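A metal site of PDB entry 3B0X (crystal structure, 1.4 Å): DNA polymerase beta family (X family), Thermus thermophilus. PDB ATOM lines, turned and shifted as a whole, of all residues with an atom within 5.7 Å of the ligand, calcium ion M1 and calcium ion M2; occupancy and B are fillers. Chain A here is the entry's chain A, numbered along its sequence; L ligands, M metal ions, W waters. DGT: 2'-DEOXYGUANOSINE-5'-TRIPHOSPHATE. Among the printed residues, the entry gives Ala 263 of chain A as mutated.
Calcium ion M2 is bound by OD2 of Asp 200 (2.3 Å), O1G of the ligand (2.3 Å), O2B of the ligand (2.4 Å), OD1 of Asp 198 (2.4 Å), O1A of the ligand (2.4 Å), O of Asp 198 (2.4 Å) and water W13 (2.5 Å).
O2B of the ligand sits close to N of Ser 188, 2.9 Å away.
OG of Ser 188 sits at hydrogen-bond distance from O3G of the ligand, 2.6 Å away.
O3G of the ligand is in salt-bridge range of NH2 of Arg 157.
An oxygen (O3G) of the ligand lies within hydrogen-bond range of the backbone NH (N) of Gly 197, 2.9 Å away.
NH1 of Arg 191 lies within salt-bridge range of O1B of the ligand, 3.0 Å away.
An oxygen (O3') of the ligand lies within hydrogen-bond range of the backbone carbonyl oxygen (O) of Thr 260 (3.4 Å).
O of Asp 200 is in hydrogen-bond range of N of Cys 186 (2.8 Å).
The backbone carbonyl oxygen (O) of Leu 199 is in hydrogen-bond range of the backbone NH (N) of Asp 243 (2.8 Å).
The backbone NH of Lys 193 sits at hydrogen-bond distance from the backbone carbonyl oxygen of Ser 188 (3.2 Å).
The backbone carbonyl oxygen of Thr 195 sits at hydrogen-bond distance from the guanidinium group of Arg 157 (2.9 Å).
The guanidinium group (NH1) of Arg 191 sits at hydrogen-bond distance from the backbone carbonyl oxygen (O) of Thr 260, 2.8 Å away.
The backbone carbonyl oxygen of Leu 259 sits at hydrogen-bond distance from the backbone NH of Gly 187.
OG1 of Thr 260 sits close to SG of Cys 186, 3.7 Å away.
N2 of the ligand lies close to NH1 of Arg 270, 3.1 Å away.
Residues that only touch the ligand: Tyr 258 (3.2 Å), Leu 259 (3.3 Å), Gly 187 (3.4 Å), Gly 261 (3.5 Å) and Val 196 (3.7 Å).
Hydrophobic or aromatic side chains that line the ligand: Tyr 258 and Leu 259.
Within 4 Å of the ligand: Arg 157, Gly 187, Ser 188, Arg 191, Val 196, Gly 197, Asp 198, Asp 200, Tyr 258, Leu 259, Thr 260, Gly 261 and Arg 270.
Water W9 lies within hydrogen-bond range of O1B of the ligand (2.7 Å) and NH2 of Arg 191 (2.8 Å).
Water W1 lies within hydrogen-bond range of the side-chain hydroxyl (OG) of Ser 266 (2.7 Å), the backbone carbonyl oxygen (O) of Tyr 258 (2.7 Å) and a nitrogen (N3) of the ligand (2.9 Å).
Water W11 lies within hydrogen-bond range of the guanidinium group (NH1) of Arg 270 (2.9 Å) and a nitrogen (N2) of the ligand (3.1 Å).
Water W4 lies within hydrogen-bond range of the backbone carbonyl oxygen of Ala 263 (2.9 Å), the guanidinium group of Arg 270 (3.1 Å) and a nitrogen (N2) of the ligand (3.5 Å).
Calcium ion M1 is bound by water W5 (2.3 Å), water W6 (2.4 Å), the side-chain carboxylate (OD2) of Asp 243 (2.4 Å), the side-chain carboxylate (OD1) of Asp 200 (2.4 Å), an oxygen (O1A) of the ligand (2.5 Å), the side-chain carboxylate (OD2) of Asp 198 (2.5 Å) and the side-chain carboxylate (OD1) of Asp 198 (2.5 Å).
The nearest printed residue that does not touch calcium ion M2 is Leu 199 (4.3 Å).
Within 4 Å of calcium ion M1: Asp 198, Asp 200 and Asp 243.
The nearest printed residue that does not touch calcium ion M1 is Leu 199 (5.2 Å).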
ATOM      1  N   MET A   1       0.885   8.674 -29.815  1.00  0.00           N
ATOM      2  CA  MET A   1      -0.115   9.460 -29.031  1.00  0.00           C
ATOM      3  C   MET A   1       0.533  10.280 -27.935  1.00  0.00           C
ATOM      4  O   MET A   1       1.529   9.860 -27.340  1.00  0.00           O
ATOM      5  CB  MET A   1      -1.162   8.533 -28.418  1.00  0.00           C
ATOM      6  CG  MET A   1      -2.314   8.247 -29.343  1.00  0.00           C
ATOM      7  SD  MET A   1      -3.663   7.457 -28.460  1.00  0.00           S
ATOM      8  CE  MET A   1      -3.283   5.736 -28.776  1.00  0.00           C
ATOM      9  N   ARG A 157      16.505  -0.802 -12.522  1.00  0.00           N
ATOM     10  CA  ARG A 157      16.250  -2.055 -13.255  1.00  0.00           C
ATOM     11  C   ARG A 157      16.691  -3.233 -12.407  1.00  0.00           C
ATOM     12  O   ARG A 157      17.581  -3.086 -11.578  1.00  0.00           O
ATOM     13  CB  ARG A 157      16.953  -2.027 -14.609  1.00  0.00           C
ATOM     14  CG  ARG A 157      16.616  -0.763 -15.412  1.00  0.00           C
ATOM     15  CD  ARG A 157      17.244  -0.760 -16.789  1.00  0.00           C
ATOM     16  NE  ARG A 157      16.675  -1.792 -17.652  1.00  0.00           N
ATOM     17  CZ  ARG A 157      15.534  -1.687 -18.312  1.00  0.00           C
ATOM     18  NH1 ARG A 157      14.808  -0.578 -18.256  1.00  0.00           N
ATOM     19  NH2 ARG A 157      15.127  -2.681 -19.081  1.00  0.00           N
ATOM     20  N   CYS A 186       4.253  -9.315 -20.986  1.00  0.00           N
ATOM     21  CA  CYS A 186       4.804  -8.697 -22.181  1.00  0.00           C
ATOM     22  C   CYS A 186       6.012  -7.820 -21.840  1.00  0.00           C
ATOM     23  O   CYS A 186       6.847  -8.207 -21.015  1.00  0.00           O
ATOM     24  CB  CYS A 186       3.690  -7.968 -22.953  1.00  0.00           C
ATOM     25  SG  CYS A 186       2.374  -9.082 -23.538  1.00  0.00           S
ATOM     26  N   GLY A 187       6.119  -6.658 -22.469  1.00  0.00           N
ATOM     27  CA  GLY A 187       7.234  -5.745 -22.270  1.00  0.00           C
ATOM     28  C   GLY A 187       8.578  -6.402 -22.511  1.00  0.00           C
ATOM     29  O   GLY A 187       8.711  -7.432 -23.199  1.00  0.00           O
ATOM     30  N   SER A 188       9.610  -5.812 -21.917  1.00  0.00           N
ATOM     31  CA  SER A 188      10.993  -6.274 -22.138  1.00  0.00           C
ATOM     32  C   SER A 188      11.229  -7.679 -21.557  1.00  0.00           C
ATOM     33  O   SER A 188      12.097  -8.407 -22.054  1.00  0.00           O
ATOM     34  CB  SER A 188      11.977  -5.282 -21.563  1.00  0.00           C
ATOM     35  OG  SER A 188      11.759  -5.157 -20.169  1.00  0.00           O
ATOM     36  N   ALA A 189      10.418  -8.090 -20.574  1.00  0.00           N
ATOM     37  CA  ALA A 189      10.541  -9.435 -20.033  1.00  0.00           C
ATOM     38  C   ALA A 189      10.249 -10.481 -21.107  1.00  0.00           C
ATOM     39  O   ALA A 189      10.956 -11.486 -21.200  1.00  0.00           O
ATOM     40  CB  ALA A 189       9.627  -9.640 -18.842  1.00  0.00           C
ATOM     41  N   ARG A 191      10.769 -10.198 -24.156  1.00  0.00           N
ATOM     42  CA  ARG A 191      11.888 -10.151 -25.092  1.00  0.00           C
ATOM     43  C   ARG A 191      13.179 -10.731 -24.487  1.00  0.00           C
ATOM     44  O   ARG A 191      14.213 -10.735 -25.156  1.00  0.00           O
ATOM     45  CB  ARG A 191      12.130  -8.738 -25.610  1.00  0.00           C
ATOM     46  CG  ARG A 191      10.857  -8.071 -26.168  1.00  0.00           C
ATOM     47  CD  ARG A 191      11.169  -6.898 -27.083  1.00  0.00           C
ATOM     48  NE  ARG A 191      12.090  -5.930 -26.490  1.00  0.00           N
ATOM     49  CZ  ARG A 191      11.759  -4.948 -25.651  1.00  0.00           C
ATOM     50  NH1 ARG A 191      10.500  -4.725 -25.276  1.00  0.00           N
ATOM     51  NH2 ARG A 191      12.733  -4.166 -25.134  1.00  0.00           N
ATOM     52  N   LYS A 193      15.124  -9.509 -22.263  1.00  0.00           N
ATOM     53  CA  LYS A 193      16.128  -8.505 -21.907  1.00  0.00           C
ATOM     54  C   LYS A 193      16.678  -8.814 -20.530  1.00  0.00           C
ATOM     55  O   LYS A 193      15.917  -9.227 -19.649  1.00  0.00           O
ATOM     56  CB  LYS A 193      15.483  -7.143 -21.931  1.00  0.00           C
ATOM     57  CG  LYS A 193      16.491  -6.005 -21.986  1.00  0.00           C
ATOM     58  CD  LYS A 193      15.776  -4.673 -22.159  1.00  0.00           C
ATOM     59  CE  LYS A 193      16.744  -3.506 -22.122  1.00  0.00           C
ATOM     60  NZ  LYS A 193      17.473  -3.453 -23.431  1.00  0.00           N
ATOM     61  N   THR A 195      17.882  -7.117 -17.996  1.00  0.00           N
ATOM     62  CA  THR A 195      17.389  -6.334 -16.870  1.00  0.00           C
ATOM     63  C   THR A 195      16.090  -5.719 -17.340  1.00  0.00           C
ATOM     64  O   THR A 195      15.912  -5.444 -18.537  1.00  0.00           O
ATOM     65  CB  THR A 195      18.350  -5.232 -16.390  1.00  0.00           C
ATOM     66  OG1 THR A 195      18.437  -4.179 -17.353  1.00  0.00           O
ATOM     67  CG2 THR A 195      19.740  -5.807 -16.070  1.00  0.00           C
ATOM     68  N   VAL A 196      15.178  -5.497 -16.403  1.00  0.00           N
ATOM     69  CA  VAL A 196      13.849  -4.996 -16.725  1.00  0.00           C
ATOM     70  C   VAL A 196      13.480  -3.841 -15.830  1.00  0.00           C
ATOM     71  O   VAL A 196      13.891  -3.791 -14.660  1.00  0.00           O
ATOM     72  CB  VAL A 196      12.776  -6.105 -16.659  1.00  0.00           C
ATOM     73  CG1 VAL A 196      13.070  -7.187 -17.687  1.00  0.00           C
ATOM     74  CG2 VAL A 196      12.683  -6.688 -15.241  1.00  0.00           C
ATOM     75  N   GLY A 197      12.670  -2.941 -16.370  1.00  0.00           N
ATOM     76  CA  GLY A 197      12.008  -1.905 -15.569  1.00  0.00           C
ATOM     77  C   GLY A 197      10.736  -2.489 -15.015  1.00  0.00           C
ATOM     78  O   GLY A 197      10.718  -3.579 -14.447  1.00  0.00           O
ATOM     79  N   ASP A 198       9.633  -1.764 -15.164  1.00  0.00           N
ATOM     80  CA  ASP A 198       8.355  -2.298 -14.703  1.00  0.00           C
ATOM     81  C   ASP A 198       7.922  -3.533 -15.511  1.00  0.00           C
ATOM     82  O   ASP A 198       8.475  -3.817 -16.583  1.00  0.00           O
ATOM     83  CB  ASP A 198       7.261  -1.226 -14.661  1.00  0.00           C
ATOM     84  CG  ASP A 198       6.861  -0.722 -16.042  1.00  0.00           C
ATOM     85  OD1 ASP A 198       7.180  -1.343 -17.080  1.00  0.00           O
ATOM     86  OD2 ASP A 198       6.201   0.329 -16.109  1.00  0.00           O
ATOM     87  N   LEU A 199       6.985  -4.296 -14.944  1.00  0.00           N
ATOM     88  CA  LEU A 199       6.441  -5.467 -15.638  1.00  0.00           C
ATOM     89  C   LEU A 199       5.113  -5.114 -16.250  1.00  0.00           C
ATOM     90  O   LEU A 199       4.346  -4.372 -15.650  1.00  0.00           O
ATOM     91  CB  LEU A 199       6.268  -6.617 -14.667  1.00  0.00           C
ATOM     92  CG  LEU A 199       7.647  -7.078 -14.166  1.00  0.00           C
ATOM     93  CD1 LEU A 199       7.438  -7.816 -12.879  1.00  0.00           C
ATOM     94  CD2 LEU A 199       8.412  -7.927 -15.149  1.00  0.00           C
ATOM     95  N   ASP A 200       4.850  -5.619 -17.459  1.00  0.00           N
ATOM     96  CA  ASP A 200       3.675  -5.225 -18.224  1.00  0.00           C
ATOM     97  C   ASP A 200       2.887  -6.459 -18.585  1.00  0.00           C
ATOM     98  O   ASP A 200       3.459  -7.393 -19.169  1.00  0.00           O
ATOM     99  CB  ASP A 200       4.130  -4.534 -19.515  1.00  0.00           C
ATOM    100  CG  ASP A 200       5.090  -3.431 -19.234  1.00  0.00           C
ATOM    101  OD1 ASP A 200       4.622  -2.315 -18.972  1.00  0.00           O
ATOM    102  OD2 ASP A 200       6.309  -3.677 -19.252  1.00  0.00           O
ATOM    103  N   ASP A 243       2.269  -2.735 -14.719  1.00  0.00           N
ATOM    104  CA  ASP A 243       1.276  -2.155 -15.578  1.00  0.00           C
ATOM    105  C   ASP A 243       0.402  -3.268 -16.157  1.00  0.00           C
ATOM    106  O   ASP A 243       0.902  -4.322 -16.581  1.00  0.00           O
ATOM    107  CB  ASP A 243       1.935  -1.466 -16.766  1.00  0.00           C
ATOM    108  CG  ASP A 243       2.600  -0.168 -16.413  1.00  0.00           C
ATOM    109  OD1 ASP A 243       2.337   0.440 -15.362  1.00  0.00           O
ATOM    110  OD2 ASP A 243       3.425   0.295 -17.246  1.00  0.00           O
ATOM    111  N   TYR A 258       1.729  -4.819 -29.437  1.00  0.00           N
ATOM    112  CA  TYR A 258       1.865  -3.495 -28.860  1.00  0.00           C
ATOM    113  C   TYR A 258       2.665  -3.533 -27.551  1.00  0.00           C
ATOM    114  O   TYR A 258       3.618  -2.766 -27.351  1.00  0.00           O
ATOM    115  CB  TYR A 258       0.482  -2.881 -28.651  1.00  0.00           C
ATOM    116  CG  TYR A 258       0.536  -1.545 -27.985  1.00  0.00           C
ATOM    117  CD1 TYR A 258       0.579  -0.371 -28.736  1.00  0.00           C
ATOM    118  CD2 TYR A 258       0.570  -1.444 -26.597  1.00  0.00           C
ATOM    119  CE1 TYR A 258       0.660   0.873 -28.107  1.00  0.00           C
ATOM    120  CE2 TYR A 258       0.661  -0.219 -25.956  1.00  0.00           C
ATOM    121  CZ  TYR A 258       0.695   0.931 -26.719  1.00  0.00           C
ATOM    122  OH  TYR A 258       0.775   2.165 -26.105  1.00  0.00           O
ATOM    123  N   LEU A 259       2.221  -4.370 -26.624  1.00  0.00           N
ATOM    124  CA  LEU A 259       2.800  -4.331 -25.289  1.00  0.00           C
ATOM    125  C   LEU A 259       4.156  -5.024 -25.174  1.00  0.00           C
ATOM    126  O   LEU A 259       4.876  -4.863 -24.171  1.00  0.00           O
ATOM    127  CB  LEU A 259       1.806  -4.889 -24.269  1.00  0.00           C
ATOM    128  CG  LEU A 259       2.046  -4.473 -22.819  1.00  0.00           C
ATOM    129  CD1 LEU A 259       2.138  -3.000 -22.661  1.00  0.00           C
ATOM    130  CD2 LEU A 259       0.993  -5.082 -21.915  1.00  0.00           C
ATOM    131  N   THR A 260       4.522  -5.791 -26.197  1.00  0.00           N
ATOM    132  CA  THR A 260       5.832  -6.464 -26.216  1.00  0.00           C
ATOM    133  C   THR A 260       6.922  -5.570 -26.781  1.00  0.00           C
ATOM    134  O   THR A 260       8.079  -5.661 -26.376  1.00  0.00           O
ATOM    135  CB  THR A 260       5.732  -7.795 -26.987  1.00  0.00           C
ATOM    136  OG1 THR A 260       4.803  -8.645 -26.290  1.00  0.00           O
ATOM    137  CG2 THR A 260       7.061  -8.516 -27.092  1.00  0.00           C
ATOM    138  N   GLY A 261       6.549  -4.700 -27.711  1.00  0.00           N
ATOM    139  CA  GLY A 261       7.524  -3.810 -28.325  1.00  0.00           C
ATOM    140  C   GLY A 261       8.656  -4.607 -28.963  1.00  0.00           C
ATOM    141  O   GLY A 261       8.442  -5.686 -29.494  1.00  0.00           O
ATOM    142  N   SER A 262       9.896  -4.098 -28.951  1.00  0.00           N
ATOM    143  CA  SER A 262      10.249  -2.782 -28.450  1.00  0.00           C
ATOM    144  C   SER A 262       9.515  -1.670 -29.201  1.00  0.00           C
ATOM    145  O   SER A 262       8.935  -1.888 -30.288  1.00  0.00           O
ATOM    146  CB  SER A 262      11.736  -2.590 -28.628  1.00  0.00           C
ATOM    147  OG  SER A 262      12.054  -2.402 -30.004  1.00  0.00           O
ATOM    148  N   ALA A 263       9.553  -0.464 -28.664  1.00  0.00           N
ATOM    149  CA  ALA A 263       8.951   0.679 -29.349  1.00  0.00           C
ATOM    150  C   ALA A 263       9.534   0.839 -30.748  1.00  0.00           C
ATOM    151  O   ALA A 263       8.785   1.143 -31.693  1.00  0.00           O
ATOM    152  CB  ALA A 263       9.122   1.967 -28.532  1.00  0.00           C
ATOM    153  N   SER A 266       7.921  -1.642 -33.078  1.00  0.00           N
ATOM    154  CA  SER A 266       6.563  -1.245 -33.423  1.00  0.00           C
ATOM    155  C   SER A 266       6.520  -0.085 -34.421  1.00  0.00           C
ATOM    156  O   SER A 266       5.653  -0.047 -35.299  1.00  0.00           O
ATOM    157  CB  SER A 266       5.756  -0.879 -32.190  1.00  0.00           C
ATOM    158  OG  SER A 266       5.682  -1.998 -31.356  1.00  0.00           O
ATOM    159  N   ARG A 270       4.323  -0.310 -37.835  1.00  0.00           N
ATOM    160  CA  ARG A 270       3.268   0.648 -38.180  1.00  0.00           C
ATOM    161  C   ARG A 270       3.482   1.261 -39.573  1.00  0.00           C
ATOM    162  O   ARG A 270       2.510   1.524 -40.308  1.00  0.00           O
ATOM    163  CB  ARG A 270       3.127   1.752 -37.136  1.00  0.00           C
ATOM    164  CG  ARG A 270       2.494   1.274 -35.836  1.00  0.00           C
ATOM    165  CD  ARG A 270       1.998   2.453 -35.000  1.00  0.00           C
ATOM    166  NE  ARG A 270       3.090   3.357 -34.699  1.00  0.00           N
ATOM    167  CZ  ARG A 270       3.951   3.205 -33.696  1.00  0.00           C
ATOM    168  NH1 ARG A 270       3.844   2.191 -32.859  1.00  0.00           N
ATOM    169  NH2 ARG A 270       4.927   4.094 -33.552  1.00  0.00           N
HETATM  170  PG  DGT L   1      11.526  -1.594 -19.649  1.00  0.00           P
HETATM  171  O1G DGT L   1      10.241  -1.471 -18.863  1.00  0.00           O
HETATM  172  O2G DGT L   1      12.387  -0.351 -19.690  1.00  0.00           O
HETATM  173  O3G DGT L   1      12.365  -2.809 -19.260  1.00  0.00           O
HETATM  174  O3B DGT L   1      11.156  -1.895 -21.201  1.00  0.00           O
HETATM  175  PB  DGT L   1       9.718  -2.170 -21.838  1.00  0.00           P
HETATM  176  O1B DGT L   1       9.929  -2.506 -23.277  1.00  0.00           O
HETATM  177  O2B DGT L   1       8.912  -3.109 -21.001  1.00  0.00           O
HETATM  178  O3A DGT L   1       9.054  -0.703 -21.805  1.00  0.00           O
HETATM  179  PA  DGT L   1       7.740  -0.050 -21.153  1.00  0.00           P
HETATM  180  O1A DGT L   1       7.345  -0.767 -19.908  1.00  0.00           O
HETATM  181  O2A DGT L   1       8.010   1.434 -21.075  1.00  0.00           O
HETATM  182  O5' DGT L   1       6.633  -0.212 -22.273  1.00  0.00           O
HETATM  183  C5' DGT L   1       6.108  -1.531 -22.548  1.00  0.00           C
HETATM  184  C4' DGT L   1       5.833  -1.687 -24.030  1.00  0.00           C
HETATM  185  O4' DGT L   1       4.839  -0.745 -24.407  1.00  0.00           O
HETATM  186  C3' DGT L   1       6.986  -1.403 -24.958  1.00  0.00           C
HETATM  187  O3' DGT L   1       7.862  -2.509 -25.122  1.00  0.00           O
HETATM  188  C2' DGT L   1       6.303  -1.056 -26.253  1.00  0.00           C
HETATM  189  C1' DGT L   1       5.041  -0.355 -25.769  1.00  0.00           C
HETATM  190  N9  DGT L   1       5.204   1.102 -25.802  1.00  0.00           N
HETATM  191  C8  DGT L   1       5.818   1.863 -24.859  1.00  0.00           C
HETATM  192  N7  DGT L   1       5.775   3.165 -25.231  1.00  0.00           N
HETATM  193  C5  DGT L   1       5.118   3.218 -26.403  1.00  0.00           C
HETATM  194  C6  DGT L   1       4.727   4.286 -27.341  1.00  0.00           C
HETATM  195  O6  DGT L   1       4.994   5.481 -27.096  1.00  0.00           O
HETATM  196  N1  DGT L   1       4.066   3.911 -28.436  1.00  0.00           N
HETATM  197  C2  DGT L   1       3.764   2.620 -28.715  1.00  0.00           C
HETATM  198  N2  DGT L   1       3.107   2.347 -29.847  1.00  0.00           N
HETATM  199  N3  DGT L   1       4.097   1.571 -27.930  1.00  0.00           N
HETATM  200  C4  DGT L   1       4.746   1.848 -26.767  1.00  0.00           C
HETATM  201 CA    CA M   1       5.434  -0.149 -18.432  1.00  0.00          CA
HETATM  202 CA    CA M   2       8.281  -2.678 -18.737  1.00  0.00          CA
HETATM  203  O   HOH W   1       4.702  -1.010 -29.091  1.00  0.00           O
HETATM  204  O   HOH W   2       9.902   0.527 -16.998  1.00  0.00           O
HETATM  205  O   HOH W   3      13.975  -0.417 -22.061  1.00  0.00           O
HETATM  206  O   HOH W   4       6.364   2.617 -31.094  1.00  0.00           O
HETATM  207  O   HOH W   5       6.369   1.973 -18.611  1.00  0.00           O
HETATM  208  O   HOH W   6       4.208   0.652 -20.288  1.00  0.00           O
HETATM  209  O   HOH W   7      10.086   2.588 -22.242  1.00  0.00           O
HETATM  210  O   HOH W   8       1.318   4.390 -31.068  1.00  0.00           O
HETATM  211  O   HOH W   9      12.146  -1.495 -24.426  1.00  0.00           O
HETATM  212  O   HOH W  10       3.480   5.894 -30.418  1.00  0.00           O
HETATM  213  O   HOH W  11       1.637   0.581 -31.968  1.00  0.00           O
HETATM  214  O   HOH W  12       6.260   3.430 -21.859  1.00  0.00           O
HETATM  215  O   HOH W  13       9.397  -4.964 -18.775  1.00  0.00           O
